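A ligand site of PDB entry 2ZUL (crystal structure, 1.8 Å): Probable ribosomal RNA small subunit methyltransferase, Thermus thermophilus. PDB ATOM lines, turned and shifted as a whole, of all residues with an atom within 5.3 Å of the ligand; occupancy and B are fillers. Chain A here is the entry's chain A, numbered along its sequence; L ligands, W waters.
S1 of the ligand lies close to O of Asn 305 (3.6 Å).
Merely in contact with the ligand: Phe 207, Ala 246, Ser 287, Val 318, Gly 243, Pro 306, Phe 322, Pro 307 and Leu 247.
The side-chain carboxylate (OE2) of Glu 262 is in hydrogen-bond range of the backbone NH (N) of Asp 264.
The backbone NH (N) of Ala 242 is in hydrogen-bond range of the backbone carbonyl oxygen (O) of Val 261.
N of Gly 241 is in hydrogen-bond range of O of Val 261 (2.9 Å).
The backbone NH (N) of Asp 263 lies within hydrogen-bond range of the backbone carbonyl oxygen (O) of Ser 287 (3.3 Å).
The side-chain hydroxyl (OG) of Ser 216 sits at hydrogen-bond distance from the side-chain amide nitrogen (ND2) of Asn 305 (3.2 Å).
The side-chain carboxylate (OD1) of Asp 263 sits at hydrogen-bond distance from the backbone NH (N) of Ala 77, at 2.8 Å.
N of Ser 287 lies within hydrogen-bond range of O of Glu 262 (2.9 Å).
The side-chain carboxylate of Glu 262 lies within hydrogen-bond range of the backbone NH of Gly 243, at 2.8 Å.
Water W5 lies within hydrogen-bond range of O1 of the ligand, N of Ala 246 and N of Tyr 244.
Water W1 lies within hydrogen-bond range of an oxygen (O1) of the ligand (2.8 Å), the backbone NH (N) of Asp 213 (2.9 Å) and the side-chain hydroxyl (OH) of Tyr 244 (3.0 Å).
Water W2 lies within hydrogen-bond range of the side-chain hydroxyl of Ser 267, an oxygen (O4) of the ligand and the backbone NH of Phe 207.
Water W6 lies within hydrogen-bond range of the side-chain carboxylate (OD2) of Asp 239 (2.6 Å), the backbone carbonyl oxygen (O) of Ala 242 (2.7 Å), the backbone NH (N) of Leu 247 (2.9 Å), a nitrogen (N1) of the ligand (3.0 Å) and the backbone NH (N) of Ala 246 (3.4 Å).
Water W4 lies within hydrogen-bond range of OD2 of Asp 263 (3.0 Å) and N4 of the ligand (3.1 Å).
The side-chain carboxylate (OD1) of Asp 288 is in hydrogen-bond range of a nitrogen (N4) of the ligand (3.1 Å).
OG of Ser 216 is in hydrogen-bond range of O2 of the ligand.
O of Gly 241 is in hydrogen-bond range of N1 of the ligand.
N of Asp 263 lies within hydrogen-bond range of N6 of the ligand (3.3 Å).
The side-chain hydroxyl (OH) of Tyr 8 is in hydrogen-bond range of a nitrogen (N4) of the ligand (3.4 Å).
The backbone carbonyl oxygen of Ala 242 lies close to a nitrogen (N1) of the ligand (3.5 Å).
An oxygen (O4) of the ligand lies within hydrogen-bond range of the side-chain carboxylate (OE1) of Glu 262.
The backbone NH (N) of Val 289 is in hydrogen-bond range of a nitrogen (N5) of the ligand, at 2.9 Å.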
ATOM      1  N   TYR A   8      23.359   8.296  29.294  1.00  0.00           N
ATOM      2  CA  TYR A   8      22.629   9.226  28.449  1.00  0.00           C
ATOM      3  C   TYR A   8      21.405   9.796  29.165  1.00  0.00           C
ATOM      4  O   TYR A   8      21.108  10.984  29.054  1.00  0.00           O
ATOM      5  CB  TYR A   8      22.149   8.551  27.163  1.00  0.00           C
ATOM      6  CG  TYR A   8      21.296   9.498  26.337  1.00  0.00           C
ATOM      7  CD1 TYR A   8      21.889  10.450  25.521  1.00  0.00           C
ATOM      8  CD2 TYR A   8      19.909   9.513  26.473  1.00  0.00           C
ATOM      9  CE1 TYR A   8      21.120  11.411  24.859  1.00  0.00           C
ATOM     10  CE2 TYR A   8      19.133  10.472  25.824  1.00  0.00           C
ATOM     11  CZ  TYR A   8      19.742  11.417  25.022  1.00  0.00           C
ATOM     12  OH  TYR A   8      18.993  12.395  24.429  1.00  0.00           O
ATOM     13  N   ALA A  77      13.898  16.223  26.651  1.00  0.00           N
ATOM     14  CA  ALA A  77      15.165  16.120  27.369  1.00  0.00           C
ATOM     15  C   ALA A  77      15.344  17.347  28.256  1.00  0.00           C
ATOM     16  O   ALA A  77      15.677  17.242  29.434  1.00  0.00           O
ATOM     17  CB  ALA A  77      16.319  16.004  26.382  1.00  0.00           C
ATOM     18  N   ARG A 113      16.443  25.965  14.514  1.00  0.00           N
ATOM     19  CA  ARG A 113      15.148  25.408  14.124  1.00  0.00           C
ATOM     20  C   ARG A 113      14.637  25.960  12.796  1.00  0.00           C
ATOM     21  O   ARG A 113      13.618  25.489  12.278  1.00  0.00           O
ATOM     22  CB  ARG A 113      14.117  25.674  15.233  1.00  0.00           C
ATOM     23  CG  ARG A 113      14.463  25.050  16.580  1.00  0.00           C
ATOM     24  CD  ARG A 113      14.158  23.568  16.593  1.00  0.00           C
ATOM     25  NE  ARG A 113      12.713  23.334  16.514  1.00  0.00           N
ATOM     26  CZ  ARG A 113      12.146  22.149  16.378  1.00  0.00           C
ATOM     27  NH1 ARG A 113      12.901  21.052  16.311  1.00  0.00           N
ATOM     28  NH2 ARG A 113      10.825  22.046  16.308  1.00  0.00           N
ATOM     29  N   PHE A 207      12.123  18.352  10.999  1.00  0.00           N
ATOM     30  CA  PHE A 207      13.169  17.898  10.095  1.00  0.00           C
ATOM     31  C   PHE A 207      12.519  17.643   8.732  1.00  0.00           C
ATOM     32  O   PHE A 207      11.392  17.136   8.666  1.00  0.00           O
ATOM     33  CB  PHE A 207      13.800  16.598  10.593  1.00  0.00           C
ATOM     34  CG  PHE A 207      14.684  15.918   9.585  1.00  0.00           C
ATOM     35  CD1 PHE A 207      15.959  16.382   9.321  1.00  0.00           C
ATOM     36  CD2 PHE A 207      14.213  14.806   8.885  1.00  0.00           C
ATOM     37  CE1 PHE A 207      16.761  15.762   8.359  1.00  0.00           C
ATOM     38  CE2 PHE A 207      15.015  14.186   7.923  1.00  0.00           C
ATOM     39  CZ  PHE A 207      16.289  14.664   7.660  1.00  0.00           C
ATOM     40  N   SER A 208      13.210  18.013   7.663  1.00  0.00           N
ATOM     41  CA  SER A 208      12.741  17.809   6.295  1.00  0.00           C
ATOM     42  C   SER A 208      11.338  18.330   6.027  1.00  0.00           C
ATOM     43  O   SER A 208      10.479  17.610   5.502  1.00  0.00           O
ATOM     44  CB  SER A 208      12.820  16.316   5.935  1.00  0.00           C
ATOM     45  OG  SER A 208      12.572  16.119   4.552  1.00  0.00           O
ATOM     46  N   ASP A 213      12.284  13.114   3.123  1.00  0.00           N
ATOM     47  CA  ASP A 213      13.733  13.075   3.000  1.00  0.00           C
ATOM     48  C   ASP A 213      14.175  11.837   2.219  1.00  0.00           C
ATOM     49  O   ASP A 213      13.685  10.739   2.453  1.00  0.00           O
ATOM     50  CB  ASP A 213      14.398  13.045   4.380  1.00  0.00           C
ATOM     51  CG  ASP A 213      15.901  13.178   4.291  1.00  0.00           C
ATOM     52  OD1 ASP A 213      16.381  14.299   4.031  1.00  0.00           O
ATOM     53  OD2 ASP A 213      16.587  12.147   4.462  1.00  0.00           O
ATOM     54  N   SER A 216      15.073   8.712   4.253  1.00  0.00           N
ATOM     55  CA  SER A 216      13.941   7.991   4.827  1.00  0.00           C
ATOM     56  C   SER A 216      13.340   7.054   3.796  1.00  0.00           C
ATOM     57  O   SER A 216      12.978   5.919   4.091  1.00  0.00           O
ATOM     58  CB  SER A 216      12.874   8.979   5.312  1.00  0.00           C
ATOM     59  OG  SER A 216      13.435   9.909   6.225  1.00  0.00           O
ATOM     60  N   ASP A 239       9.940   3.587  16.166  1.00  0.00           N
ATOM     61  CA  ASP A 239      10.551   4.549  15.248  1.00  0.00           C
ATOM     62  C   ASP A 239      11.275   5.585  16.099  1.00  0.00           C
ATOM     63  O   ASP A 239      10.653   6.444  16.713  1.00  0.00           O
ATOM     64  CB  ASP A 239       9.458   5.207  14.389  1.00  0.00           C
ATOM     65  CG  ASP A 239      10.016   6.195  13.376  1.00  0.00           C
ATOM     66  OD1 ASP A 239      11.237   6.412  13.346  1.00  0.00           O
ATOM     67  OD2 ASP A 239       9.205   6.763  12.608  1.00  0.00           O
ATOM     68  N   LEU A 240      12.604   5.491  16.147  1.00  0.00           N
ATOM     69  CA  LEU A 240      13.424   6.410  16.951  1.00  0.00           C
ATOM     70  C   LEU A 240      13.612   7.745  16.235  1.00  0.00           C
ATOM     71  O   LEU A 240      14.279   7.812  15.193  1.00  0.00           O
ATOM     72  CB  LEU A 240      14.786   5.755  17.244  1.00  0.00           C
ATOM     73  CG  LEU A 240      14.770   4.519  18.140  1.00  0.00           C
ATOM     74  CD1 LEU A 240      16.128   3.816  18.097  1.00  0.00           C
ATOM     75  CD2 LEU A 240      14.424   4.931  19.569  1.00  0.00           C
ATOM     76  N   GLY A 241      13.023   8.805  16.789  1.00  0.00           N
ATOM     77  CA  GLY A 241      13.109  10.128  16.187  1.00  0.00           C
ATOM     78  C   GLY A 241      12.132  10.146  15.022  1.00  0.00           C
ATOM     79  O   GLY A 241      12.527  10.397  13.883  1.00  0.00           O
ATOM     80  N   ALA A 242      10.858   9.929  15.328  1.00  0.00           N
ATOM     81  CA  ALA A 242       9.810   9.835  14.311  1.00  0.00           C
ATOM     82  C   ALA A 242       9.483  11.070  13.488  1.00  0.00           C
ATOM     83  O   ALA A 242       8.938  10.935  12.394  1.00  0.00           O
ATOM     84  CB  ALA A 242       8.530   9.293  14.962  1.00  0.00           C
ATOM     85  N   GLY A 243       9.776  12.261  14.004  1.00  0.00           N
ATOM     86  CA  GLY A 243       9.478  13.477  13.258  1.00  0.00           C
ATOM     87  C   GLY A 243       8.003  13.555  12.925  1.00  0.00           C
ATOM     88  O   GLY A 243       7.169  13.154  13.726  1.00  0.00           O
ATOM     89  N   TYR A 244       7.665  14.080  11.746  1.00  0.00           N
ATOM     90  CA  TYR A 244       6.257  14.168  11.369  1.00  0.00           C
ATOM     91  C   TYR A 244       5.717  12.844  10.821  1.00  0.00           C
ATOM     92  O   TYR A 244       4.582  12.785  10.363  1.00  0.00           O
ATOM     93  CB  TYR A 244       6.019  15.319  10.380  1.00  0.00           C
ATOM     94  CG  TYR A 244       6.790  15.247   9.084  1.00  0.00           C
ATOM     95  CD1 TYR A 244       6.450  14.315   8.092  1.00  0.00           C
ATOM     96  CD2 TYR A 244       7.839  16.124   8.833  1.00  0.00           C
ATOM     97  CE1 TYR A 244       7.148  14.270   6.891  1.00  0.00           C
ATOM     98  CE2 TYR A 244       8.539  16.087   7.626  1.00  0.00           C
ATOM     99  CZ  TYR A 244       8.183  15.158   6.665  1.00  0.00           C
ATOM    100  OH  TYR A 244       8.884  15.112   5.481  1.00  0.00           O
ATOM    101  N   ALA A 246       7.589  10.397   8.472  1.00  0.00           N
ATOM    102  CA  ALA A 246       8.016   9.926   7.156  1.00  0.00           C
ATOM    103  C   ALA A 246       8.104   8.403   7.131  1.00  0.00           C
ATOM    104  O   ALA A 246       7.776   7.758   6.135  1.00  0.00           O
ATOM    105  CB  ALA A 246       9.361  10.533   6.787  1.00  0.00           C
ATOM    106  N   LEU A 247       8.558   7.817   8.243  1.00  0.00           N
ATOM    107  CA  LEU A 247       8.683   6.370   8.359  1.00  0.00           C
ATOM    108  C   LEU A 247       7.468   5.785   9.085  1.00  0.00           C
ATOM    109  O   LEU A 247       6.997   4.697   8.755  1.00  0.00           O
ATOM    110  CB  LEU A 247       9.945   6.004   9.152  1.00  0.00           C
ATOM    111  CG  LEU A 247      11.294   6.517   8.652  1.00  0.00           C
ATOM    112  CD1 LEU A 247      12.389   6.024   9.582  1.00  0.00           C
ATOM    113  CD2 LEU A 247      11.539   6.017   7.231  1.00  0.00           C
ATOM    114  N   VAL A 261       8.858   7.670  18.921  1.00  0.00           N
ATOM    115  CA  VAL A 261       9.338   8.505  20.020  1.00  0.00           C
ATOM    116  C   VAL A 261      10.014   9.706  19.375  1.00  0.00           C
ATOM    117  O   VAL A 261      10.772   9.559  18.414  1.00  0.00           O
ATOM    118  CB  VAL A 261      10.305   7.743  20.961  1.00  0.00           C
ATOM    119  CG1 VAL A 261       9.531   6.686  21.743  1.00  0.00           C
ATOM    120  CG2 VAL A 261      11.444   7.101  20.176  1.00  0.00           C
ATOM    121  N   GLU A 262       9.710  10.887  19.890  1.00  0.00           N
ATOM    122  CA  GLU A 262      10.233  12.130  19.341  1.00  0.00           C
ATOM    123  C   GLU A 262      10.403  13.156  20.459  1.00  0.00           C
ATOM    124  O   GLU A 262       9.492  13.383  21.249  1.00  0.00           O
ATOM    125  CB  GLU A 262       9.254  12.638  18.272  1.00  0.00           C
ATOM    126  CG  GLU A 262       9.508  14.022  17.708  1.00  0.00           C
ATOM    127  CD  GLU A 262      10.885  14.177  17.095  1.00  0.00           C
ATOM    128  OE1 GLU A 262      11.223  13.406  16.172  1.00  0.00           O
ATOM    129  OE2 GLU A 262      11.623  15.079  17.535  1.00  0.00           O
ATOM    130  N   ASP A 263      11.587  13.776  20.513  1.00  0.00           N
ATOM    131  CA  ASP A 263      11.893  14.749  21.567  1.00  0.00           C
ATOM    132  C   ASP A 263      11.260  16.114  21.373  1.00  0.00           C
ATOM    133  O   ASP A 263      11.019  16.832  22.353  1.00  0.00           O
ATOM    134  CB  ASP A 263      13.412  14.922  21.684  1.00  0.00           C
ATOM    135  CG  ASP A 263      13.813  15.702  22.919  1.00  0.00           C
ATOM    136  OD1 ASP A 263      13.560  15.215  24.043  1.00  0.00           O
ATOM    137  OD2 ASP A 263      14.390  16.813  22.778  1.00  0.00           O
ATOM    138  N   ASP A 264      10.998  16.488  20.123  1.00  0.00           N
ATOM    139  CA  ASP A 264      10.435  17.801  19.798  1.00  0.00           C
ATOM    140  C   ASP A 264       8.904  17.839  19.775  1.00  0.00           C
ATOM    141  O   ASP A 264       8.268  17.140  18.990  1.00  0.00           O
ATOM    142  CB  ASP A 264      10.986  18.269  18.447  1.00  0.00           C
ATOM    143  CG  ASP A 264      10.410  19.611  18.015  1.00  0.00           C
ATOM    144  OD1 ASP A 264      10.569  20.592  18.763  1.00  0.00           O
ATOM    145  OD2 ASP A 264       9.809  19.663  16.925  1.00  0.00           O
ATOM    146  N   SER A 267       7.153  18.474  16.454  1.00  0.00           N
ATOM    147  CA  SER A 267       7.199  17.292  15.607  1.00  0.00           C
ATOM    148  C   SER A 267       6.200  16.237  16.060  1.00  0.00           C
ATOM    149  O   SER A 267       5.605  15.539  15.240  1.00  0.00           O
ATOM    150  CB  SER A 267       8.611  16.712  15.600  1.00  0.00           C
ATOM    151  OG  SER A 267       9.528  17.661  15.051  1.00  0.00           O
ATOM    152  N   SER A 287       9.056  12.002  23.742  1.00  0.00           N
ATOM    153  CA  SER A 287       9.996  11.303  24.597  1.00  0.00           C
ATOM    154  C   SER A 287      11.457  11.569  24.250  1.00  0.00           C
ATOM    155  O   SER A 287      11.798  11.796  23.087  1.00  0.00           O
ATOM    156  CB  SER A 287       9.695   9.798  24.474  1.00  0.00           C
ATOM    157  OG  SER A 287      10.669   8.973  25.098  1.00  0.00           O
ATOM    158  N   ASP A 288      12.315  11.553  25.275  1.00  0.00           N
ATOM    159  CA  ASP A 288      13.757  11.733  25.082  1.00  0.00           C
ATOM    160  C   ASP A 288      14.208  10.306  24.824  1.00  0.00           C
ATOM    161  O   ASP A 288      14.370   9.510  25.757  1.00  0.00           O
ATOM    162  CB  ASP A 288      14.391  12.280  26.364  1.00  0.00           C
ATOM    163  CG  ASP A 288      15.897  12.466  26.244  1.00  0.00           C
ATOM    164  OD1 ASP A 288      16.427  12.372  25.111  1.00  0.00           O
ATOM    165  OD2 ASP A 288      16.546  12.729  27.280  1.00  0.00           O
ATOM    166  N   VAL A 289      14.394   9.981  23.548  1.00  0.00           N
ATOM    167  CA  VAL A 289      14.763   8.634  23.115  1.00  0.00           C
ATOM    168  C   VAL A 289      13.672   7.697  23.673  1.00  0.00           C
ATOM    169  O   VAL A 289      12.489   7.910  23.396  1.00  0.00           O
ATOM    170  CB  VAL A 289      16.176   8.224  23.595  1.00  0.00           C
ATOM    171  CG1 VAL A 289      16.613   6.933  22.917  1.00  0.00           C
ATOM    172  CG2 VAL A 289      17.175   9.314  23.227  1.00  0.00           C
ATOM    173  N   ASN A 305      16.251   7.197  11.343  1.00  0.00           N
ATOM    174  CA  ASN A 305      17.023   8.090  10.490  1.00  0.00           C
ATOM    175  C   ASN A 305      17.394   9.055  11.615  1.00  0.00           C
ATOM    176  O   ASN A 305      16.673  10.022  11.889  1.00  0.00           O
ATOM    177  CB  ASN A 305      16.138   8.788   9.463  1.00  0.00           C
ATOM    178  CG  ASN A 305      16.911   9.806   8.642  1.00  0.00           C
ATOM    179  OD1 ASN A 305      18.111  10.012   8.873  1.00  0.00           O
ATOM    180  ND2 ASN A 305      16.241  10.458   7.702  1.00  0.00           N
ATOM    181  N   PRO A 306      18.507   8.785  12.296  1.00  0.00           N
ATOM    182  CA  PRO A 306      18.988   9.597  13.417  1.00  0.00           C
ATOM    183  C   PRO A 306      19.404  11.017  13.084  1.00  0.00           C
ATOM    184  O   PRO A 306      19.785  11.324  11.945  1.00  0.00           O
ATOM    185  CB  PRO A 306      20.169   8.789  13.965  1.00  0.00           C
ATOM    186  CG  PRO A 306      19.927   7.396  13.455  1.00  0.00           C
ATOM    187  CD  PRO A 306      19.417   7.646  12.063  1.00  0.00           C
ATOM    188  N   PRO A 307      19.325  11.911  14.083  1.00  0.00           N
ATOM    189  CA  PRO A 307      19.711  13.304  13.875  1.00  0.00           C
ATOM    190  C   PRO A 307      21.186  13.327  13.478  1.00  0.00           C
ATOM    191  O   PRO A 307      21.916  12.356  13.734  1.00  0.00           O
ATOM    192  CB  PRO A 307      19.456  13.943  15.238  1.00  0.00           C
ATOM    193  CG  PRO A 307      19.628  12.796  16.201  1.00  0.00           C
ATOM    194  CD  PRO A 307      18.932  11.666  15.480  1.00  0.00           C
ATOM    195  N   PHE A 308      21.629  14.405  12.857  1.00  0.00           N
ATOM    196  CA  PHE A 308      23.021  14.515  12.437  1.00  0.00           C
ATOM    197  C   PHE A 308      23.417  15.966  12.226  1.00  0.00           C
ATOM    198  O   PHE A 308      22.561  16.828  12.027  1.00  0.00           O
ATOM    199  CB  PHE A 308      23.226  13.723  11.141  1.00  0.00           C
ATOM    200  CG  PHE A 308      22.469  14.260   9.965  1.00  0.00           C
ATOM    201  CD1 PHE A 308      23.029  15.246   9.144  1.00  0.00           C
ATOM    202  CD2 PHE A 308      21.185  13.810   9.675  1.00  0.00           C
ATOM    203  CE1 PHE A 308      22.313  15.764   8.066  1.00  0.00           C
ATOM    204  CE2 PHE A 308      20.459  14.328   8.593  1.00  0.00           C
ATOM    205  CZ  PHE A 308      21.035  15.306   7.787  1.00  0.00           C
ATOM    206  N   VAL A 318      22.953  11.853  20.841  1.00  0.00           N
ATOM    207  CA  VAL A 318      21.607  11.318  20.724  1.00  0.00           C
ATOM    208  C   VAL A 318      21.556  10.155  19.735  1.00  0.00           C
ATOM    209  O   VAL A 318      20.867   9.153  19.977  1.00  0.00           O
ATOM    210  CB  VAL A 318      20.608  12.405  20.258  1.00  0.00           C
ATOM    211  CG1 VAL A 318      19.235  11.797  20.046  1.00  0.00           C
ATOM    212  CG2 VAL A 318      20.529  13.501  21.308  1.00  0.00           C
ATOM    213  N   PHE A 322      20.489   6.247  20.226  1.00  0.00           N
ATOM    214  CA  PHE A 322      19.483   5.584  19.393  1.00  0.00           C
ATOM    215  C   PHE A 322      19.940   4.150  19.145  1.00  0.00           C
ATOM    216  O   PHE A 322      19.157   3.202  19.259  1.00  0.00           O
ATOM    217  CB  PHE A 322      19.336   6.310  18.066  1.00  0.00           C
ATOM    218  CG  PHE A 322      18.329   7.433  18.072  1.00  0.00           C
ATOM    219  CD1 PHE A 322      17.955   8.057  19.252  1.00  0.00           C
ATOM    220  CD2 PHE A 322      17.771   7.884  16.866  1.00  0.00           C
ATOM    221  CE1 PHE A 322      17.053   9.117  19.256  1.00  0.00           C
ATOM    222  CE2 PHE A 322      16.867   8.945  16.853  1.00  0.00           C
ATOM    223  CZ  PHE A 322      16.508   9.562  18.048  1.00  0.00           C
HETATM  224  N1  LIG L   1      12.060   9.934  11.194  1.00  0.00           N
HETATM  225  C1  LIG L   1      11.869  11.267  10.605  1.00  0.00           C
HETATM  226  C2  LIG L   1      12.120  11.197   9.093  1.00  0.00           C
HETATM  227  O1  LIG L   1      11.776  12.183   8.412  1.00  0.00           O
HETATM  228  O2  LIG L   1      12.657  10.150   8.659  1.00  0.00           O
HETATM  229  C3  LIG L   1      12.836  12.264  11.247  1.00  0.00           C
HETATM  230  C4  LIG L   1      14.182  12.233  10.928  1.00  0.00           C
HETATM  231  S1  LIG L   1      15.307  13.372  11.645  1.00  0.00           S
HETATM  232  C5  LIG L   1      16.882  13.250  10.824  1.00  0.00           C
HETATM  233  C6  LIG L   1      15.767  12.904  13.350  1.00  0.00           C
HETATM  234  C7  LIG L   1      14.626  13.041  14.354  1.00  0.00           C
HETATM  235  O3  LIG L   1      15.139  12.727  15.659  1.00  0.00           O
HETATM  236  C8  LIG L   1      14.126  14.488  14.422  1.00  0.00           C
HETATM  237  O4  LIG L   1      12.699  14.518  14.436  1.00  0.00           O
HETATM  238  C9  LIG L   1      14.660  14.963  15.772  1.00  0.00           C
HETATM  239  O5  LIG L   1      13.765  15.939  16.319  1.00  0.00           O
HETATM  240  C10 LIG L   1      14.516  13.661  16.555  1.00  0.00           C
HETATM  241  N2  LIG L   1      15.235  13.702  17.844  1.00  0.00           N
HETATM  242  C11 LIG L   1      16.291  14.481  18.134  1.00  0.00           C
HETATM  243  N3  LIG L   1      16.680  14.246  19.387  1.00  0.00           N
HETATM  244  C12 LIG L   1      15.884  13.318  19.896  1.00  0.00           C
HETATM  245  C13 LIG L   1      15.793  12.680  21.131  1.00  0.00           C
HETATM  246  N4  LIG L   1      16.639  13.001  22.108  1.00  0.00           N
HETATM  247  N5  LIG L   1      14.844  11.766  21.324  1.00  0.00           N
HETATM  248  C14 LIG L   1      13.986  11.463  20.368  1.00  0.00           C
HETATM  249  N6  LIG L   1      14.028  12.042  19.189  1.00  0.00           N
HETATM  250  C15 LIG L   1      14.962  12.969  18.917  1.00  0.00           C
HETATM  251  O   HOH W   1      11.102  13.125   5.815  1.00  0.00           O
HETATM  252  O   HOH W   2      11.240  16.600  13.143  1.00  0.00           O
HETATM  253  O   HOH W   3      14.766  17.772  18.249  1.00  0.00           O
HETATM  254  O   HOH W   4      17.218  15.985  22.467  1.00  0.00           O
HETATM  255  O   HOH W   5       9.196  12.686   9.165  1.00  0.00           O
HETATM  256  O   HOH W   6       9.335   8.780  10.900  1.00  0.00           O
HETATM  257  O   HOH W   7      13.511   7.914  12.499  1.00  0.00           O
